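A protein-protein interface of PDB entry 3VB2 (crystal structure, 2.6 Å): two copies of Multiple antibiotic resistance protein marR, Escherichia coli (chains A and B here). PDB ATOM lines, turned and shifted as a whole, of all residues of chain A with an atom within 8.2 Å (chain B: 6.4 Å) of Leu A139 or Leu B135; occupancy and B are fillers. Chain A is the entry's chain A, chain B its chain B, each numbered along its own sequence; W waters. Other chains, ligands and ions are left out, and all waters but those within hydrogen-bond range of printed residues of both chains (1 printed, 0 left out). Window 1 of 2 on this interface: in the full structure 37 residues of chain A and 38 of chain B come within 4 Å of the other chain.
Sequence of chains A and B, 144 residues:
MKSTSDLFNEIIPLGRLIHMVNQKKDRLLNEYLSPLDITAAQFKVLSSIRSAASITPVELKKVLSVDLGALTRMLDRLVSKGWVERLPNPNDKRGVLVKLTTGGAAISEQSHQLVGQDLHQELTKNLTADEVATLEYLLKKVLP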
ATOM      1  N   ILE A  12      -5.364  15.656 -19.277  1.00  0.00           N
ATOM      2  CA  ILE A  12      -4.480  16.797 -19.460  1.00  0.00           C
ATOM      3  C   ILE A  12      -3.232  16.606 -18.622  1.00  0.00           C
ATOM      4  O   ILE A  12      -3.326  16.247 -17.440  1.00  0.00           O
ATOM      5  CB  ILE A  12      -5.183  18.104 -19.049  1.00  0.00           C
ATOM      6  CG1 ILE A  12      -6.562  18.183 -19.703  1.00  0.00           C
ATOM      7  CG2 ILE A  12      -4.334  19.318 -19.414  1.00  0.00           C
ATOM      8  CD1 ILE A  12      -7.360  19.403 -19.316  1.00  0.00           C
ATOM      9  N   LEU A  14       0.089  17.129 -16.323  1.00  0.00           N
ATOM     10  CA  LEU A  14       0.313  17.900 -15.137  1.00  0.00           C
ATOM     11  C   LEU A  14       0.790  19.346 -15.456  1.00  0.00           C
ATOM     12  O   LEU A  14       0.202  20.320 -14.969  1.00  0.00           O
ATOM     13  CB  LEU A  14       1.320  17.172 -14.228  1.00  0.00           C
ATOM     14  CG  LEU A  14       1.675  17.809 -12.890  1.00  0.00           C
ATOM     15  CD1 LEU A  14       0.421  18.244 -12.126  1.00  0.00           C
ATOM     16  CD2 LEU A  14       2.506  16.834 -12.077  1.00  0.00           C
ATOM     17  N   GLY A  15       1.834  19.466 -16.289  1.00  0.00           N
ATOM     18  CA  GLY A  15       2.413  20.778 -16.631  1.00  0.00           C
ATOM     19  C   GLY A  15       1.364  21.749 -17.123  1.00  0.00           C
ATOM     20  O   GLY A  15       1.289  22.884 -16.669  1.00  0.00           O
ATOM     21  N   LEU A  17      -2.020  21.499 -16.663  1.00  0.00           N
ATOM     22  CA  LEU A  17      -2.885  21.783 -15.513  1.00  0.00           C
ATOM     23  C   LEU A  17      -2.328  22.852 -14.591  1.00  0.00           C
ATOM     24  O   LEU A  17      -3.077  23.723 -14.120  1.00  0.00           O
ATOM     25  CB  LEU A  17      -3.166  20.516 -14.711  1.00  0.00           C
ATOM     26  CG  LEU A  17      -4.044  19.476 -15.403  1.00  0.00           C
ATOM     27  CD1 LEU A  17      -4.130  18.213 -14.570  1.00  0.00           C
ATOM     28  CD2 LEU A  17      -5.428  20.038 -15.684  1.00  0.00           C
ATOM     29  N   ILE A  18      -1.031  22.754 -14.273  1.00  0.00           N
ATOM     30  CA  ILE A  18      -0.359  23.768 -13.407  1.00  0.00           C
ATOM     31  C   ILE A  18      -0.468  25.154 -14.029  1.00  0.00           C
ATOM     32  O   ILE A  18      -0.721  26.128 -13.348  1.00  0.00           O
ATOM     33  CB  ILE A  18       1.130  23.431 -13.206  1.00  0.00           C
ATOM     34  CG1 ILE A  18       1.277  22.196 -12.332  1.00  0.00           C
ATOM     35  CG2 ILE A  18       1.877  24.620 -12.612  1.00  0.00           C
ATOM     36  CD1 ILE A  18       2.571  21.451 -12.566  1.00  0.00           C
ATOM     37  N   VAL A  21      -4.255  26.430 -13.878  1.00  0.00           N
ATOM     38  CA  VAL A  21      -4.586  26.819 -12.501  1.00  0.00           C
ATOM     39  C   VAL A  21      -3.834  28.098 -12.069  1.00  0.00           C
ATOM     40  O   VAL A  21      -4.373  28.945 -11.330  1.00  0.00           O
ATOM     41  CB  VAL A  21      -4.283  25.671 -11.492  1.00  0.00           C
ATOM     42  CG1 VAL A  21      -4.579  26.116 -10.062  1.00  0.00           C
ATOM     43  CG2 VAL A  21      -5.092  24.431 -11.845  1.00  0.00           C
ATOM     44  N   VAL A 132      -8.379  19.975  -0.226  1.00  0.00           N
ATOM     45  CA  VAL A 132      -7.430  21.106  -0.188  1.00  0.00           C
ATOM     46  C   VAL A 132      -6.108  20.662   0.448  1.00  0.00           C
ATOM     47  O   VAL A 132      -5.036  20.903  -0.111  1.00  0.00           O
ATOM     48  CB  VAL A 132      -8.008  22.342   0.579  1.00  0.00           C
ATOM     49  CG1 VAL A 132      -6.940  23.428   0.743  1.00  0.00           C
ATOM     50  CG2 VAL A 132      -9.212  22.902  -0.143  1.00  0.00           C
ATOM     51  N   ALA A 133      -6.192  19.985   1.601  1.00  0.00           N
ATOM     52  CA  ALA A 133      -4.985  19.483   2.286  1.00  0.00           C
ATOM     53  C   ALA A 133      -4.181  18.508   1.404  1.00  0.00           C
ATOM     54  O   ALA A 133      -2.932  18.581   1.360  1.00  0.00           O
ATOM     55  CB  ALA A 133      -5.343  18.835   3.616  1.00  0.00           C
ATOM     56  N   THR A 134      -4.892  17.622   0.680  1.00  0.00           N
ATOM     57  CA  THR A 134      -4.247  16.694  -0.243  1.00  0.00           C
ATOM     58  C   THR A 134      -3.586  17.417  -1.428  1.00  0.00           C
ATOM     59  O   THR A 134      -2.438  17.118  -1.782  1.00  0.00           O
ATOM     60  CB  THR A 134      -5.229  15.602  -0.773  1.00  0.00           C
ATOM     61  OG1 THR A 134      -5.756  14.860   0.324  1.00  0.00           O
ATOM     62  CG2 THR A 134      -4.502  14.632  -1.712  1.00  0.00           C
ATOM     63  N   LEU A 135      -4.317  18.348  -2.056  1.00  0.00           N
ATOM     64  CA  LEU A 135      -3.770  19.086  -3.201  1.00  0.00           C
ATOM     65  C   LEU A 135      -2.505  19.826  -2.808  1.00  0.00           C
ATOM     66  O   LEU A 135      -1.500  19.777  -3.522  1.00  0.00           O
ATOM     67  CB  LEU A 135      -4.794  20.048  -3.769  1.00  0.00           C
ATOM     68  CG  LEU A 135      -4.357  20.970  -4.923  1.00  0.00           C
ATOM     69  CD1 LEU A 135      -3.877  20.173  -6.123  1.00  0.00           C
ATOM     70  CD2 LEU A 135      -5.501  21.884  -5.318  1.00  0.00           C
ATOM     71  N   GLU A 136      -2.541  20.470  -1.646  1.00  0.00           N
ATOM     72  CA  GLU A 136      -1.380  21.171  -1.110  1.00  0.00           C
ATOM     73  C   GLU A 136      -0.231  20.219  -0.851  1.00  0.00           C
ATOM     74  O   GLU A 136       0.907  20.486  -1.233  1.00  0.00           O
ATOM     75  CB  GLU A 136      -1.748  21.924   0.184  1.00  0.00           C
ATOM     76  CG  GLU A 136      -2.493  23.242  -0.062  1.00  0.00           C
ATOM     77  CD  GLU A 136      -3.094  23.858   1.218  1.00  0.00           C
ATOM     78  OE1 GLU A 136      -3.010  23.215   2.317  1.00  0.00           O
ATOM     79  OE2 GLU A 136      -3.641  24.999   1.127  1.00  0.00           O
ATOM     80  N   TYR A 137      -0.535  19.103  -0.210  1.00  0.00           N
ATOM     81  CA  TYR A 137       0.451  18.105   0.077  1.00  0.00           C
ATOM     82  C   TYR A 137       1.187  17.669  -1.216  1.00  0.00           C
ATOM     83  O   TYR A 137       2.414  17.694  -1.280  1.00  0.00           O
ATOM     84  CB  TYR A 137      -0.208  16.912   0.751  1.00  0.00           C
ATOM     85  CG  TYR A 137       0.717  15.761   0.982  1.00  0.00           C
ATOM     86  CD1 TYR A 137       1.799  15.871   1.876  1.00  0.00           C
ATOM     87  CD2 TYR A 137       0.529  14.535   0.308  1.00  0.00           C
ATOM     88  CE1 TYR A 137       2.669  14.804   2.083  1.00  0.00           C
ATOM     89  CE2 TYR A 137       1.385  13.459   0.519  1.00  0.00           C
ATOM     90  CZ  TYR A 137       2.454  13.592   1.402  1.00  0.00           C
ATOM     91  OH  TYR A 137       3.297  12.520   1.614  1.00  0.00           O
ATOM     92  N   LEU A 138       0.416  17.313  -2.247  1.00  0.00           N
ATOM     93  CA  LEU A 138       0.980  16.757  -3.472  1.00  0.00           C
ATOM     94  C   LEU A 138       1.742  17.812  -4.295  1.00  0.00           C
ATOM     95  O   LEU A 138       2.769  17.494  -4.952  1.00  0.00           O
ATOM     96  CB  LEU A 138      -0.115  16.069  -4.320  1.00  0.00           C
ATOM     97  CG  LEU A 138      -0.842  14.862  -3.628  1.00  0.00           C
ATOM     98  CD1 LEU A 138      -2.018  14.362  -4.451  1.00  0.00           C
ATOM     99  CD2 LEU A 138       0.117  13.726  -3.317  1.00  0.00           C
ATOM    100  N   LEU A 139       1.289  19.074  -4.228  1.00  0.00           N
ATOM    101  CA  LEU A 139       1.995  20.154  -4.908  1.00  0.00           C
ATOM    102  C   LEU A 139       3.355  20.391  -4.260  1.00  0.00           C
ATOM    103  O   LEU A 139       4.366  20.589  -4.964  1.00  0.00           O
ATOM    104  CB  LEU A 139       1.173  21.436  -4.932  1.00  0.00           C
ATOM    105  CG  LEU A 139       0.042  21.554  -5.980  1.00  0.00           C
ATOM    106  CD1 LEU A 139      -0.862  22.746  -5.655  1.00  0.00           C
ATOM    107  CD2 LEU A 139       0.607  21.662  -7.402  1.00  0.00           C
ATOM    108  N   LYS A 140       3.400  20.308  -2.919  1.00  0.00           N
ATOM    109  CA  LYS A 140       4.674  20.341  -2.186  1.00  0.00           C
ATOM    110  C   LYS A 140       5.641  19.215  -2.668  1.00  0.00           C
ATOM    111  O   LYS A 140       6.837  19.442  -2.820  1.00  0.00           O
ATOM    112  CB  LYS A 140       4.439  20.216  -0.681  1.00  0.00           C
ATOM    113  CG  LYS A 140       3.711  21.385  -0.044  1.00  0.00           C
ATOM    114  CD  LYS A 140       4.133  21.547   1.406  1.00  0.00           C
ATOM    115  CE  LYS A 140       2.956  21.880   2.327  1.00  0.00           C
ATOM    116  NZ  LYS A 140       1.944  20.772   2.443  1.00  0.00           N
ATOM    117  N   LYS A 141       5.087  18.014  -2.914  1.00  0.00           N
ATOM    118  CA  LYS A 141       5.887  16.834  -3.339  1.00  0.00           C
ATOM    119  C   LYS A 141       6.540  16.996  -4.728  1.00  0.00           C
ATOM    120  O   LYS A 141       7.509  16.334  -5.037  1.00  0.00           O
ATOM    121  CB  LYS A 141       5.031  15.563  -3.309  1.00  0.00           C
ATOM    122  CG  LYS A 141       5.109  14.777  -2.003  1.00  0.00           C
ATOM    123  CD  LYS A 141       4.543  13.388  -2.171  1.00  0.00           C
ATOM    124  CE  LYS A 141       5.148  12.428  -1.181  1.00  0.00           C
ATOM    125  NZ  LYS A 141       5.006  11.013  -1.633  1.00  0.00           N
ATOM    126  N   VAL A 142       5.971  17.859  -5.557  1.00  0.00           N
ATOM    127  CA  VAL A 142       6.528  18.148  -6.885  1.00  0.00           C
ATOM    128  C   VAL A 142       7.773  19.064  -6.787  1.00  0.00           C
ATOM    129  O   VAL A 142       8.617  19.069  -7.681  1.00  0.00           O
ATOM    130  CB  VAL A 142       5.454  18.819  -7.811  1.00  0.00           C
ATOM    131  CG1 VAL A 142       6.107  19.522  -8.988  1.00  0.00           C
ATOM    132  CG2 VAL A 142       4.452  17.793  -8.300  1.00  0.00           C
ATOM    133  N   LEU A 143       7.882  19.811  -5.681  1.00  0.00           N
ATOM    134  CA  LEU A 143       8.850  20.922  -5.578  1.00  0.00           C
ATOM    135  C   LEU A 143      10.301  20.488  -5.315  1.00  0.00           C
ATOM    136  O   LEU A 143      11.248  21.131  -5.811  1.00  0.00           O
ATOM    137  CB  LEU A 143       8.402  21.931  -4.534  1.00  0.00           C
ATOM    138  CG  LEU A 143       7.279  22.855  -4.986  1.00  0.00           C
ATOM    139  CD1 LEU A 143       6.692  23.600  -3.803  1.00  0.00           C
ATOM    140  CD2 LEU A 143       7.778  23.821  -6.057  1.00  0.00           C
ATOM    141  N   PRO A 144      10.490  19.409  -4.537  1.00  0.00           N
ATOM    142  CA  PRO A 144      11.844  18.850  -4.426  1.00  0.00           C
ATOM    143  C   PRO A 144      12.318  18.228  -5.770  1.00  0.00           C
ATOM    144  O   PRO A 144      11.497  17.799  -6.611  1.00  0.00           O
ATOM    145  CB  PRO A 144      11.688  17.751  -3.340  1.00  0.00           C
ATOM    146  CG  PRO A 144      10.437  18.118  -2.598  1.00  0.00           C
ATOM    147  CD  PRO A 144       9.541  18.756  -3.615  1.00  0.00           C
ATOM    148  OXT PRO A 144      13.527  18.155  -6.052  1.00  0.00           O
ATOM    149  N   LEU B   7       9.297  22.130   3.565  1.00  0.00           N
ATOM    150  CA  LEU B   7       7.976  22.398   3.021  1.00  0.00           C
ATOM    151  C   LEU B   7       6.887  21.574   3.734  1.00  0.00           C
ATOM    152  O   LEU B   7       5.753  22.029   3.888  1.00  0.00           O
ATOM    153  CB  LEU B   7       7.947  22.094   1.504  1.00  0.00           C
ATOM    154  CG  LEU B   7       9.051  22.686   0.593  1.00  0.00           C
ATOM    155  CD1 LEU B   7      10.442  22.182   0.982  1.00  0.00           C
ATOM    156  CD2 LEU B   7       8.764  22.370  -0.867  1.00  0.00           C
ATOM    157  N   LEU B  14      -2.093  27.419  -0.553  1.00  0.00           N
ATOM    158  CA  LEU B  14      -2.270  26.796  -1.835  1.00  0.00           C
ATOM    159  C   LEU B  14      -1.832  27.706  -3.025  1.00  0.00           C
ATOM    160  O   LEU B  14      -1.210  27.239  -3.983  1.00  0.00           O
ATOM    161  CB  LEU B  14      -3.722  26.371  -2.001  1.00  0.00           C
ATOM    162  CG  LEU B  14      -4.135  25.854  -3.381  1.00  0.00           C
ATOM    163  CD1 LEU B  14      -3.316  24.635  -3.754  1.00  0.00           C
ATOM    164  CD2 LEU B  14      -5.616  25.522  -3.388  1.00  0.00           C
ATOM    165  N   LEU B  17       1.862  27.719  -3.327  1.00  0.00           N
ATOM    166  CA  LEU B  17       2.304  26.435  -3.882  1.00  0.00           C
ATOM    167  C   LEU B  17       2.125  26.388  -5.389  1.00  0.00           C
ATOM    168  O   LEU B  17       3.033  25.959  -6.128  1.00  0.00           O
ATOM    169  CB  LEU B  17       1.555  25.286  -3.232  1.00  0.00           C
ATOM    170  CG  LEU B  17       1.935  24.989  -1.794  1.00  0.00           C
ATOM    171  CD1 LEU B  17       1.025  23.915  -1.233  1.00  0.00           C
ATOM    172  CD2 LEU B  17       3.414  24.582  -1.705  1.00  0.00           C
ATOM    173  N   ILE B  18       0.954  26.822  -5.849  1.00  0.00           N
ATOM    174  CA  ILE B  18       0.633  26.840  -7.277  1.00  0.00           C
ATOM    175  C   ILE B  18       1.631  27.695  -8.035  1.00  0.00           C
ATOM    176  O   ILE B  18       2.039  27.359  -9.146  1.00  0.00           O
ATOM    177  CB  ILE B  18      -0.782  27.413  -7.520  1.00  0.00           C
ATOM    178  CG1 ILE B  18      -1.846  26.441  -7.021  1.00  0.00           C
ATOM    179  CG2 ILE B  18      -0.992  27.726  -8.995  1.00  0.00           C
ATOM    180  CD1 ILE B  18      -3.147  27.117  -6.643  1.00  0.00           C
ATOM    181  N   VAL B  21       5.279  25.866  -7.982  1.00  0.00           N
ATOM    182  CA  VAL B  21       5.234  24.712  -8.923  1.00  0.00           C
ATOM    183  C   VAL B  21       5.160  25.185 -10.395  1.00  0.00           C
ATOM    184  O   VAL B  21       5.716  24.544 -11.306  1.00  0.00           O
ATOM    185  CB  VAL B  21       4.037  23.778  -8.609  1.00  0.00           C
ATOM    186  CG1 VAL B  21       3.853  22.738  -9.710  1.00  0.00           C
ATOM    187  CG2 VAL B  21       4.237  23.108  -7.255  1.00  0.00           C
ATOM    188  N   LEU B 123       8.523  16.406 -13.428  1.00  0.00           N
ATOM    189  CA  LEU B 123       7.526  16.949 -12.488  1.00  0.00           C
ATOM    190  C   LEU B 123       7.010  15.897 -11.508  1.00  0.00           C
ATOM    191  O   LEU B 123       6.726  16.207 -10.343  1.00  0.00           O
ATOM    192  CB  LEU B 123       6.337  17.540 -13.251  1.00  0.00           C
ATOM    193  CG  LEU B 123       6.484  18.923 -13.893  1.00  0.00           C
ATOM    194  CD1 LEU B 123       5.158  19.365 -14.473  1.00  0.00           C
ATOM    195  CD2 LEU B 123       7.028  19.969 -12.916  1.00  0.00           C
ATOM    196  N   THR B 124       6.833  14.667 -12.000  1.00  0.00           N
ATOM    197  CA  THR B 124       6.211  13.609 -11.224  1.00  0.00           C
ATOM    198  C   THR B 124       7.222  12.640 -10.598  1.00  0.00           C
ATOM    199  O   THR B 124       6.830  11.610 -10.037  1.00  0.00           O
ATOM    200  CB  THR B 124       5.219  12.788 -12.074  1.00  0.00           C
ATOM    201  OG1 THR B 124       5.926  12.135 -13.139  1.00  0.00           O
ATOM    202  CG2 THR B 124       4.149  13.672 -12.653  1.00  0.00           C
ATOM    203  N   LEU B 127       6.468  11.560  -7.171  1.00  0.00           N
ATOM    204  CA  LEU B 127       5.074  11.139  -6.968  1.00  0.00           C
ATOM    205  C   LEU B 127       4.879   9.682  -7.297  1.00  0.00           C
ATOM    206  O   LEU B 127       5.506   9.145  -8.240  1.00  0.00           O
ATOM    207  CB  LEU B 127       4.123  11.979  -7.816  1.00  0.00           C
ATOM    208  CG  LEU B 127       4.050  13.486  -7.536  1.00  0.00           C
ATOM    209  CD1 LEU B 127       2.788  14.067  -8.164  1.00  0.00           C
ATOM    210  CD2 LEU B 127       4.084  13.760  -6.047  1.00  0.00           C
ATOM    211  N   ASP B 130      -0.513   6.859  -8.368  1.00  0.00           N
ATOM    212  CA  ASP B 130      -1.829   7.279  -7.902  1.00  0.00           C
ATOM    213  C   ASP B 130      -1.812   8.707  -7.329  1.00  0.00           C
ATOM    214  O   ASP B 130      -2.832   9.400  -7.336  1.00  0.00           O
ATOM    215  CB  ASP B 130      -2.413   6.280  -6.882  1.00  0.00           C
ATOM    216  CG  ASP B 130      -1.530   6.099  -5.663  1.00  0.00           C
ATOM    217  OD1 ASP B 130      -0.746   5.137  -5.635  1.00  0.00           O
ATOM    218  OD2 ASP B 130      -1.642   6.892  -4.718  1.00  0.00           O
ATOM    219  N   GLU B 131      -0.649   9.142  -6.847  1.00  0.00           N
ATOM    220  CA  GLU B 131      -0.472  10.530  -6.469  1.00  0.00           C
ATOM    221  C   GLU B 131      -0.552  11.466  -7.672  1.00  0.00           C
ATOM    222  O   GLU B 131      -1.129  12.559  -7.580  1.00  0.00           O
ATOM    223  CB  GLU B 131       0.823  10.730  -5.708  1.00  0.00           C
ATOM    224  CG  GLU B 131       0.716  10.310  -4.256  1.00  0.00           C
ATOM    225  CD  GLU B 131       2.043  10.345  -3.523  1.00  0.00           C
ATOM    226  OE1 GLU B 131       2.022  10.485  -2.276  1.00  0.00           O
ATOM    227  OE2 GLU B 131       3.107  10.211  -4.184  1.00  0.00           O
ATOM    228  N   VAL B 132      -0.027  11.018  -8.808  1.00  0.00           N
ATOM    229  CA  VAL B 132      -0.148  11.781 -10.058  1.00  0.00           C
ATOM    230  C   VAL B 132      -1.601  11.889 -10.474  1.00  0.00           C
ATOM    231  O   VAL B 132      -2.066  12.964 -10.848  1.00  0.00           O
ATOM    232  CB  VAL B 132       0.693  11.155 -11.227  1.00  0.00           C
ATOM    233  CG1 VAL B 132       0.499  11.954 -12.502  1.00  0.00           C
ATOM    234  CG2 VAL B 132       2.163  11.106 -10.861  1.00  0.00           C
ATOM    235  N   ALA B 133      -2.325  10.781 -10.377  1.00  0.00           N
ATOM    236  CA  ALA B 133      -3.743  10.750 -10.775  1.00  0.00           C
ATOM    237  C   ALA B 133      -4.595  11.622  -9.853  1.00  0.00           C
ATOM    238  O   ALA B 133      -5.488  12.334 -10.314  1.00  0.00           O
ATOM    239  CB  ALA B 133      -4.275   9.305 -10.802  1.00  0.00           C
ATOM    240  N   THR B 134      -4.298  11.580  -8.555  1.00  0.00           N
ATOM    241  CA  THR B 134      -4.993  12.436  -7.577  1.00  0.00           C
ATOM    242  C   THR B 134      -4.693  13.924  -7.797  1.00  0.00           C
ATOM    243  O   THR B 134      -5.587  14.752  -7.718  1.00  0.00           O
ATOM    244  CB  THR B 134      -4.632  12.075  -6.109  1.00  0.00           C
ATOM    245  OG1 THR B 134      -4.884  10.700  -5.872  1.00  0.00           O
ATOM    246  CG2 THR B 134      -5.457  12.902  -5.140  1.00  0.00           C
ATOM    247  N   LEU B 135      -3.426  14.253  -8.008  1.00  0.00           N
ATOM    248  CA  LEU B 135      -3.027  15.646  -8.234  1.00  0.00           C
ATOM    249  C   LEU B 135      -3.700  16.205  -9.486  1.00  0.00           C
ATOM    250  O   LEU B 135      -4.238  17.314  -9.469  1.00  0.00           O
ATOM    251  CB  LEU B 135      -1.502  15.759  -8.354  1.00  0.00           C
ATOM    252  CG  LEU B 135      -0.908  17.157  -8.653  1.00  0.00           C
ATOM    253  CD1 LEU B 135      -1.307  18.200  -7.578  1.00  0.00           C
ATOM    254  CD2 LEU B 135       0.618  17.076  -8.815  1.00  0.00           C
ATOM    255  N   GLU B 136      -3.707  15.414 -10.557  1.00  0.00           N
ATOM    256  CA  GLU B 136      -4.380  15.806 -11.800  1.00  0.00           C
ATOM    257  C   GLU B 136      -5.871  15.969 -11.593  1.00  0.00           C
ATOM    258  O   GLU B 136      -6.453  16.985 -11.971  1.00  0.00           O
ATOM    259  CB  GLU B 136      -4.107  14.798 -12.894  1.00  0.00           C
ATOM    260  CG  GLU B 136      -2.700  14.890 -13.483  1.00  0.00           C
ATOM    261  CD  GLU B 136      -2.392  13.747 -14.456  1.00  0.00           C
ATOM    262  OE1 GLU B 136      -3.295  12.883 -14.682  1.00  0.00           O
ATOM    263  OE2 GLU B 136      -1.241  13.707 -14.997  1.00  0.00           O
ATOM    264  N   TYR B 137      -6.475  15.003 -10.931  1.00  0.00           N
ATOM    265  CA  TYR B 137      -7.875  15.087 -10.563  1.00  0.00           C
ATOM    266  C   TYR B 137      -8.235  16.411  -9.834  1.00  0.00           C
ATOM    267  O   TYR B 137      -9.160  17.107 -10.223  1.00  0.00           O
ATOM    268  CB  TYR B 137      -8.255  13.906  -9.686  1.00  0.00           C
ATOM    269  CG  TYR B 137      -9.670  13.935  -9.269  1.00  0.00           C
ATOM    270  CD1 TYR B 137     -10.693  13.841 -10.214  1.00  0.00           C
ATOM    271  CD2 TYR B 137     -10.023  14.112  -7.918  1.00  0.00           C
ATOM    272  CE1 TYR B 137     -12.030  13.894  -9.832  1.00  0.00           C
ATOM    273  CE2 TYR B 137     -11.354  14.140  -7.528  1.00  0.00           C
ATOM    274  CZ  TYR B 137     -12.352  14.049  -8.498  1.00  0.00           C
ATOM    275  OH  TYR B 137     -13.651  14.079  -8.142  1.00  0.00           O
ATOM    276  N   LEU B 138      -7.497  16.723  -8.770  1.00  0.00           N
ATOM    277  CA  LEU B 138      -7.828  17.842  -7.908  1.00  0.00           C
ATOM    278  C   LEU B 138      -7.531  19.207  -8.579  1.00  0.00           C
ATOM    279  O   LEU B 138      -8.261  20.188  -8.375  1.00  0.00           O
ATOM    280  CB  LEU B 138      -7.095  17.726  -6.571  1.00  0.00           C
ATOM    281  CG  LEU B 138      -7.436  16.518  -5.690  1.00  0.00           C
ATOM    282  CD1 LEU B 138      -6.500  16.456  -4.485  1.00  0.00           C
ATOM    283  CD2 LEU B 138      -8.906  16.547  -5.240  1.00  0.00           C
ATOM    284  N   LEU B 139      -6.476  19.258  -9.377  1.00  0.00           N
ATOM    285  CA  LEU B 139      -6.203  20.433 -10.163  1.00  0.00           C
ATOM    286  C   LEU B 139      -7.346  20.726 -11.169  1.00  0.00           C
ATOM    287  O   LEU B 139      -7.727  21.896 -11.365  1.00  0.00           O
ATOM    288  CB  LEU B 139      -4.862  20.307 -10.885  1.00  0.00           C
ATOM    289  CG  LEU B 139      -3.581  20.535 -10.057  1.00  0.00           C
ATOM    290  CD1 LEU B 139      -2.365  20.101 -10.850  1.00  0.00           C
ATOM    291  CD2 LEU B 139      -3.429  22.002  -9.607  1.00  0.00           C
ATOM    292  N   LYS B 140      -7.899  19.664 -11.784  1.00  0.00           N
ATOM    293  CA  LYS B 140      -9.078  19.808 -12.694  1.00  0.00           C
ATOM    294  C   LYS B 140     -10.283  20.344 -11.943  1.00  0.00           C
ATOM    295  O   LYS B 140     -11.072  21.076 -12.493  1.00  0.00           O
ATOM    296  CB  LYS B 140      -9.451  18.456 -13.365  1.00  0.00           C
ATOM    297  CG  LYS B 140      -8.454  17.954 -14.401  1.00  0.00           C
ATOM    298  CD  LYS B 140      -9.142  17.170 -15.525  1.00  0.00           C
ATOM    299  CE  LYS B 140      -9.136  15.636 -15.295  1.00  0.00           C
ATOM    300  NZ  LYS B 140      -7.958  15.085 -14.557  1.00  0.00           N
HETATM  301  O   HOH W   1       7.622  14.911  -8.025  1.00  0.00           O
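The side-chain carboxylate (OE2) of Glu A136 is in hydrogen-bond range of the backbone NH (N) of Leu B14 (3.3 Å). NZ of Lys A141 is in salt-bridge range of OE1 of Glu B131 (3.1 Å).
The side-chain hydroxyl of Thr B134 is in hydrogen-bond range of the backbone carbonyl oxygen of Asp B130, 2.8 Å away.
Among the printed residues, pairs that only touch across the chains: Lys A140 with Leu B7, Ile A18 with Val B21, Leu A139 with Val B21, Lys A141 with Leu B127, Glu A136 with Leu B17, Val A142 with Leu B123, Leu A14 with Leu B135, Leu A135 with Leu B135, Leu A14 with Leu B139, Leu A138 with Glu B131, Leu A14 with Thr B124, Lys A140 with Leu B17, Leu A139 with Leu B14, Leu A17 with Glu B136, Val A21 with Leu B139, Leu A143 with Leu B7, Leu A143 with Val B21, Gly A15 with Leu B123, Leu A135 with Leu B138, Leu A138 with Thr B134, Leu A138 with Leu B135, Ile A18 with Leu B123, Val A21 with Ile B18, Leu A135 with Leu B14, Thr A134 with Leu B138, Leu A17 with Lys B140, Leu A14 with Glu B136, Val A142 with Leu B135, Leu A139 with Leu B135, Thr A134 with Thr B134, Leu A135 with Leu B139, Leu A17 with Leu B139 and Val A142 with Val B21.
Leu A139 touches three residues of chain B. Of the printed residues of chain B, Lys A141 touches Leu B127 (3.4 Å) and Glu B131 (3.1 Å). Printed residues of chain A within 4 Å of Leu B17: Glu A136 and Lys A140. Asp B130 touches none of the printed residues of chain A. Leu B135 touches just these residues of chain A: Leu A14, Leu A135, Leu A138, Leu A139 and Val A142. Printed residues of chain A within 4 Å of Lys B140: Leu A17 (3.9 Å). The nearest residue of chain B that does not touch Leu A139 is Ile B18 (4.1 Å).
Printed residues of chain A that touch a printed residue of chain B: Leu A14, Gly A15, Leu A17, Ile A18, Val A21, Thr A134, Leu A135, Glu A136, Leu A138, Leu A139, Lys A140, Lys A141, Val A142 and Leu A143. Hydrophobic or aromatic side chains of chain A within 4 Å of the printed part of chain B: Leu A14, Leu A17, Ile A18, Val A21, Leu A135, Leu A138, Leu A139, Val A142 and Leu A143. Among the printed residues, Asp or Glu carboxylates within 4 Å of a Lys or Arg side-chain nitrogen of the other chain: Lys A141 with Glu B131.
Leu A17 touches Leu B139, but with the chains exchanged Leu A139 does not touch Leu B17 (4.2 Å). Leu A17 touches Lys B140, and with the chains exchanged Lys A140 touches Leu B17. Val A21 touches Leu B139, and with the chains exchanged Leu A139 touches Val B21. Leu A135 touches Leu B139, and with the chains exchanged Leu A139 touches Leu B135. Positions printed for both chains: 14, 17, 18, 21, 132, 133, 134, 135, 136, 137, 138, 139 and 140. Of the 35 pairs that touch across the chains among the printed residues, 22 have their exchanged pair printed and touching as well.
Water W1 bridges O of Leu B123 and O of Lys A141.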
